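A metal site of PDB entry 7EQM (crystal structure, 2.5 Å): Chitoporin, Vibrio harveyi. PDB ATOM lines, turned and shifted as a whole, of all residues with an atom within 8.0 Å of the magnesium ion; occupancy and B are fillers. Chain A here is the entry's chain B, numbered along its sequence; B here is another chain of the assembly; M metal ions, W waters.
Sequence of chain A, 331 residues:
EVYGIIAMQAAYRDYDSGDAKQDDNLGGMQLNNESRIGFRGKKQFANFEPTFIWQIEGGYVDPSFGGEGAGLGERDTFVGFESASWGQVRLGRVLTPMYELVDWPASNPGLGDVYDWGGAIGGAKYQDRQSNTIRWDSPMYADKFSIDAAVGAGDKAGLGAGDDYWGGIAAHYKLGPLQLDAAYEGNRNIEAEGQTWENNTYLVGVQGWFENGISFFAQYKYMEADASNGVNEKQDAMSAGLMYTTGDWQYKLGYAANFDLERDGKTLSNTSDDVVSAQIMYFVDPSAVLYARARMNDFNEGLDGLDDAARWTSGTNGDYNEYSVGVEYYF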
ATOM      1  N   ARG A  93      -1.110  16.474  -2.061  1.00  0.00           N
ATOM      2  CA  ARG A  93      -1.722  17.237  -3.127  1.00  0.00           C
ATOM      3  C   ARG A  93      -0.607  18.022  -3.832  1.00  0.00           C
ATOM      4  O   ARG A  93       0.053  18.859  -3.206  1.00  0.00           O
ATOM      5  CB  ARG A  93      -2.821  18.150  -2.565  1.00  0.00           C
ATOM      6  CG  ARG A  93      -3.418  19.159  -3.540  1.00  0.00           C
ATOM      7  CD  ARG A  93      -4.608  19.905  -2.918  1.00  0.00           C
ATOM      8  NE  ARG A  93      -5.367  20.639  -3.918  1.00  0.00           N
ATOM      9  CZ  ARG A  93      -6.231  20.083  -4.765  1.00  0.00           C
ATOM     10  NH1 ARG A  93      -6.443  18.770  -4.741  1.00  0.00           N
ATOM     11  NH2 ARG A  93      -6.864  20.826  -5.644  1.00  0.00           N
ATOM     12  N   THR A  96       0.541  17.450 -11.292  1.00  0.00           N
ATOM     13  CA  THR A  96       1.021  16.334 -12.084  1.00  0.00           C
ATOM     14  C   THR A  96       2.186  16.803 -12.965  1.00  0.00           C
ATOM     15  O   THR A  96       2.306  17.996 -13.252  1.00  0.00           O
ATOM     16  CB  THR A  96      -0.076  15.721 -12.952  1.00  0.00           C
ATOM     17  OG1 THR A  96      -0.224  16.458 -14.175  1.00  0.00           O
ATOM     18  CG2 THR A  96      -1.403  15.662 -12.225  1.00  0.00           C
ATOM     19  N   ALA A 124     -11.017  12.881 -19.043  1.00  0.00           N
ATOM     20  CA  ALA A 124     -10.173  13.818 -18.290  1.00  0.00           C
ATOM     21  C   ALA A 124      -8.794  13.873 -18.953  1.00  0.00           C
ATOM     22  O   ALA A 124      -7.974  12.983 -18.736  1.00  0.00           O
ATOM     23  CB  ALA A 124     -10.058  13.386 -16.832  1.00  0.00           C
ATOM     24  N   TYR A 126      -6.147  15.519 -18.419  1.00  0.00           N
ATOM     25  CA  TYR A 126      -5.130  15.402 -17.378  1.00  0.00           C
ATOM     26  C   TYR A 126      -5.678  16.005 -16.086  1.00  0.00           C
ATOM     27  O   TYR A 126      -6.552  16.877 -16.116  1.00  0.00           O
ATOM     28  CB  TYR A 126      -3.813  16.093 -17.785  1.00  0.00           C
ATOM     29  CG  TYR A 126      -3.965  17.425 -18.508  1.00  0.00           C
ATOM     30  CD1 TYR A 126      -4.278  18.597 -17.811  1.00  0.00           C
ATOM     31  CD2 TYR A 126      -3.763  17.527 -19.894  1.00  0.00           C
ATOM     32  CE1 TYR A 126      -4.406  19.807 -18.472  1.00  0.00           C
ATOM     33  CE2 TYR A 126      -3.884  18.708 -20.549  1.00  0.00           C
ATOM     34  CZ  TYR A 126      -4.210  19.858 -19.843  1.00  0.00           C
ATOM     35  OH  TYR A 126      -4.335  21.070 -20.512  1.00  0.00           O
ATOM     36  N   GLN A 127      -5.158  15.541 -14.944  1.00  0.00           N
ATOM     37  CA  GLN A 127      -5.384  16.287 -13.715  1.00  0.00           C
ATOM     38  C   GLN A 127      -4.508  17.535 -13.706  1.00  0.00           C
ATOM     39  O   GLN A 127      -3.608  17.702 -14.538  1.00  0.00           O
ATOM     40  CB  GLN A 127      -5.092  15.412 -12.475  1.00  0.00           C
ATOM     41  CG  GLN A 127      -5.932  14.125 -12.381  1.00  0.00           C
ATOM     42  CD  GLN A 127      -7.412  14.391 -12.467  1.00  0.00           C
ATOM     43  OE1 GLN A 127      -7.955  15.241 -11.758  1.00  0.00           O
ATOM     44  NE2 GLN A 127      -8.081  13.697 -13.367  1.00  0.00           N
ATOM     45  N   ASP A 128      -4.792  18.455 -12.772  1.00  0.00           N
ATOM     46  CA  ASP A 128      -3.951  19.626 -12.644  1.00  0.00           C
ATOM     47  C   ASP A 128      -3.267  19.547 -11.288  1.00  0.00           C
ATOM     48  O   ASP A 128      -2.142  19.031 -11.184  1.00  0.00           O
ATOM     49  CB  ASP A 128      -4.748  20.924 -12.874  1.00  0.00           C
ATOM     50  CG  ASP A 128      -6.089  20.929 -12.144  1.00  0.00           C
ATOM     51  OD1 ASP A 128      -6.173  20.382 -11.023  1.00  0.00           O
ATOM     52  OD2 ASP A 128      -7.048  21.489 -12.694  1.00  0.00           O
ATOM     53  N   ARG A 129      -3.859  20.090 -10.232  1.00  0.00           N
ATOM     54  CA  ARG A 129      -3.410  19.828  -8.880  1.00  0.00           C
ATOM     55  C   ARG A 129      -4.272  18.687  -8.370  1.00  0.00           C
ATOM     56  O   ARG A 129      -5.511  18.768  -8.427  1.00  0.00           O
ATOM     57  CB  ARG A 129      -3.526  21.082  -8.002  1.00  0.00           C
ATOM     58  CG  ARG A 129      -2.951  20.896  -6.621  1.00  0.00           C
ATOM     59  CD  ARG A 129      -3.097  22.177  -5.802  1.00  0.00           C
ATOM     60  NE  ARG A 129      -2.107  23.145  -6.257  1.00  0.00           N
ATOM     61  CZ  ARG A 129      -2.383  24.157  -7.069  1.00  0.00           C
ATOM     62  NH1 ARG A 129      -3.623  24.352  -7.495  1.00  0.00           N
ATOM     63  NH2 ARG A 129      -1.408  24.979  -7.451  1.00  0.00           N
ATOM     64  N   GLN A 130      -3.635  17.618  -7.934  1.00  0.00           N
ATOM     65  CA  GLN A 130      -4.356  16.399  -7.559  1.00  0.00           C
ATOM     66  C   GLN A 130      -3.939  15.942  -6.166  1.00  0.00           C
ATOM     67  O   GLN A 130      -2.742  15.872  -5.866  1.00  0.00           O
ATOM     68  CB  GLN A 130      -4.112  15.272  -8.594  1.00  0.00           C
ATOM     69  CG  GLN A 130      -5.061  14.076  -8.471  1.00  0.00           C
ATOM     70  CD  GLN A 130      -6.477  14.399  -8.940  1.00  0.00           C
ATOM     71  OE1 GLN A 130      -6.809  15.562  -9.192  1.00  0.00           O
ATOM     72  NE2 GLN A 130      -7.310  13.365  -9.091  1.00  0.00           N
ATOM     73  N   SER A 131      -4.924  15.664  -5.324  1.00  0.00           N
ATOM     74  CA  SER A 131      -4.670  15.020  -4.041  1.00  0.00           C
ATOM     75  C   SER A 131      -4.429  13.520  -4.250  1.00  0.00           C
ATOM     76  O   SER A 131      -4.538  13.001  -5.366  1.00  0.00           O
ATOM     77  CB  SER A 131      -5.835  15.268  -3.079  1.00  0.00           C
ATOM     78  OG  SER A 131      -6.059  16.652  -2.865  1.00  0.00           O
ATOM     79  N   ALA A 153      -4.620   8.639  -7.088  1.00  0.00           N
ATOM     80  CA  ALA A 153      -6.041   8.383  -7.219  1.00  0.00           C
ATOM     81  C   ALA A 153      -6.716   9.504  -8.012  1.00  0.00           C
ATOM     82  O   ALA A 153      -6.219  10.636  -8.077  1.00  0.00           O
ATOM     83  CB  ALA A 153      -6.695   8.280  -5.834  1.00  0.00           C
ATOM     84  N   GLY A 154      -7.875   9.168  -8.587  1.00  0.00           N
ATOM     85  CA  GLY A 154      -8.670  10.128  -9.331  1.00  0.00           C
ATOM     86  C   GLY A 154      -9.566  10.965  -8.431  1.00  0.00           C
ATOM     87  O   GLY A 154      -9.632  10.780  -7.217  1.00  0.00           O
ATOM     88  N   ASP A 155     -10.276  11.901  -9.048  1.00  0.00           N
ATOM     89  CA  ASP A 155     -11.191  12.750  -8.286  1.00  0.00           C
ATOM     90  C   ASP A 155     -12.289  11.950  -7.590  1.00  0.00           C
ATOM     91  O   ASP A 155     -12.585  12.187  -6.418  1.00  0.00           O
ATOM     92  CB  ASP A 155     -11.814  13.807  -9.190  1.00  0.00           C
ATOM     93  CG  ASP A 155     -10.785  14.713  -9.849  1.00  0.00           C
ATOM     94  OD1 ASP A 155     -11.154  15.378 -10.847  1.00  0.00           O
ATOM     95  OD2 ASP A 155      -9.621  14.762  -9.347  1.00  0.00           O
ATOM     96  N   LYS A 156     -12.928  11.027  -8.301  1.00  0.00           N
ATOM     97  CA  LYS A 156     -13.999  10.276  -7.658  1.00  0.00           C
ATOM     98  C   LYS A 156     -13.447   9.363  -6.571  1.00  0.00           C
ATOM     99  O   LYS A 156     -14.022   9.279  -5.473  1.00  0.00           O
ATOM    100  CB  LYS A 156     -14.764   9.488  -8.702  1.00  0.00           C
ATOM    101  CG  LYS A 156     -15.645  10.356  -9.576  1.00  0.00           C
ATOM    102  CD  LYS A 156     -16.873   9.593 -10.083  1.00  0.00           C
ATOM    103  CE  LYS A 156     -17.819  10.553 -10.820  1.00  0.00           C
ATOM    104  NZ  LYS A 156     -17.976  11.876 -10.105  1.00  0.00           N
ATOM    105  N   ASP A 164     -11.267   5.748 -10.341  1.00  0.00           N
ATOM    106  CA  ASP A 164     -10.426   6.417 -11.314  1.00  0.00           C
ATOM    107  C   ASP A 164      -9.005   6.560 -10.760  1.00  0.00           C
ATOM    108  O   ASP A 164      -8.782   6.595  -9.542  1.00  0.00           O
ATOM    109  CB  ASP A 164     -11.016   7.780 -11.688  1.00  0.00           C
ATOM    110  CG  ASP A 164     -11.543   8.581 -10.484  1.00  0.00           C
ATOM    111  OD1 ASP A 164     -11.575   8.052  -9.347  1.00  0.00           O
ATOM    112  OD2 ASP A 164     -11.918   9.761 -10.659  1.00  0.00           O
ATOM    113  N   TRP A 166      -4.617   7.642 -12.260  1.00  0.00           N
ATOM    114  CA  TRP A 166      -3.857   8.321 -13.307  1.00  0.00           C
ATOM    115  C   TRP A 166      -2.386   8.158 -13.003  1.00  0.00           C
ATOM    116  O   TRP A 166      -1.989   7.897 -11.862  1.00  0.00           O
ATOM    117  CB  TRP A 166      -4.239   9.815 -13.391  1.00  0.00           C
ATOM    118  CG  TRP A 166      -3.888  10.531 -12.130  1.00  0.00           C
ATOM    119  CD1 TRP A 166      -4.687  10.686 -11.016  1.00  0.00           C
ATOM    120  CD2 TRP A 166      -2.632  11.132 -11.806  1.00  0.00           C
ATOM    121  NE1 TRP A 166      -4.001  11.360 -10.037  1.00  0.00           N
ATOM    122  CE2 TRP A 166      -2.732  11.632 -10.489  1.00  0.00           C
ATOM    123  CE3 TRP A 166      -1.422  11.287 -12.507  1.00  0.00           C
ATOM    124  CZ2 TRP A 166      -1.681  12.309  -9.866  1.00  0.00           C
ATOM    125  CZ3 TRP A 166      -0.375  11.961 -11.875  1.00  0.00           C
ATOM    126  CH2 TRP A 166      -0.517  12.462 -10.574  1.00  0.00           C
ATOM    127  N   GLU A 185       0.528  11.840 -19.733  1.00  0.00           N
ATOM    128  CA  GLU A 185      -0.345  11.505 -18.617  1.00  0.00           C
ATOM    129  C   GLU A 185      -1.402  10.530 -19.097  1.00  0.00           C
ATOM    130  O   GLU A 185      -1.939  10.675 -20.196  1.00  0.00           O
ATOM    131  CB  GLU A 185      -1.004  12.735 -17.986  1.00  0.00           C
ATOM    132  CG  GLU A 185      -1.717  12.380 -16.666  1.00  0.00           C
ATOM    133  CD  GLU A 185      -1.964  13.589 -15.776  1.00  0.00           C
ATOM    134  OE1 GLU A 185      -1.038  14.424 -15.636  1.00  0.00           O
ATOM    135  OE2 GLU A 185      -3.099  13.695 -15.247  1.00  0.00           O
ATOM    136  N   ASN A 187      -5.060   8.857 -17.840  1.00  0.00           N
ATOM    137  CA  ASN A 187      -6.175   8.791 -16.907  1.00  0.00           C
ATOM    138  C   ASN A 187      -7.029   7.563 -17.203  1.00  0.00           C
ATOM    139  O   ASN A 187      -7.396   7.323 -18.361  1.00  0.00           O
ATOM    140  CB  ASN A 187      -7.036  10.047 -16.963  1.00  0.00           C
ATOM    141  CG  ASN A 187      -6.528  11.138 -16.064  1.00  0.00           C
ATOM    142  OD1 ASN A 187      -7.024  11.303 -14.938  1.00  0.00           O
ATOM    143  ND2 ASN A 187      -5.534  11.910 -16.531  1.00  0.00           N
ATOM    144  N   GLU B  68      -9.990  18.677  -0.294  1.00  0.00           N
ATOM    145  CA  GLU B  68      -8.895  19.439   0.283  1.00  0.00           C
ATOM    146  C   GLU B  68      -9.410  20.719   0.954  1.00  0.00           C
ATOM    147  O   GLU B  68     -10.522  21.169   0.701  1.00  0.00           O
ATOM    148  CB  GLU B  68      -7.863  19.785  -0.799  1.00  0.00           C
ATOM    149  CG  GLU B  68      -8.280  20.907  -1.747  1.00  0.00           C
ATOM    150  CD  GLU B  68      -9.165  20.433  -2.902  1.00  0.00           C
ATOM    151  OE1 GLU B  68      -9.580  19.256  -2.940  1.00  0.00           O
ATOM    152  OE2 GLU B  68      -9.437  21.260  -3.802  1.00  0.00           O
HETATM  153 MG    MG M   1      -8.428  16.346 -10.016  1.00  0.00          MG
HETATM  154  O   HOH W   1      -9.424  17.226  -8.462  1.00  0.00           O
HETATM  155  O   HOH W   2      -9.698  17.344 -11.051  1.00  0.00           O
HETATM  156  O   HOH W   3      -7.096  17.877 -10.467  1.00  0.00           O
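Water W3 lies within hydrogen-bond range of the side-chain carboxylate (OD1) of Asp 128 and the backbone carbonyl oxygen (O) of Arg 129.
Of the 18 residues printed, 3 come within 4 Å of the magnesium ion.
The nearest printed residue that does not touch the magnesium ion is Arg 129 (4.1 Å).
The magnesium ion is bound by water W2 (1.9 Å), the side-chain amide oxygen of Gln 130 (2.0 Å), water W1 (2.0 Å), water W3 (2.1 Å), the side-chain carboxylate of Asp 155 (2.1 Å) and the side-chain amide oxygen of Gln 127 (2.1 Å).
The side-chain amide nitrogen (NE2) of Gln 130 sits at hydrogen-bond distance from the backbone carbonyl oxygen (O) of Ala 153 (3.1 Å).
The backbone NH (N) of Asp 155 lies within hydrogen-bond range of the side-chain carboxylate (OD2) of Asp 164 (3.1 Å).
OD1 of Asn 187 is in hydrogen-bond range of NE2 of Gln 127 (3.1 Å).
The side-chain carboxylate (OE2) of Glu 185 is in hydrogen-bond range of the backbone NH (N) of Gln 127, at 2.8 Å.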
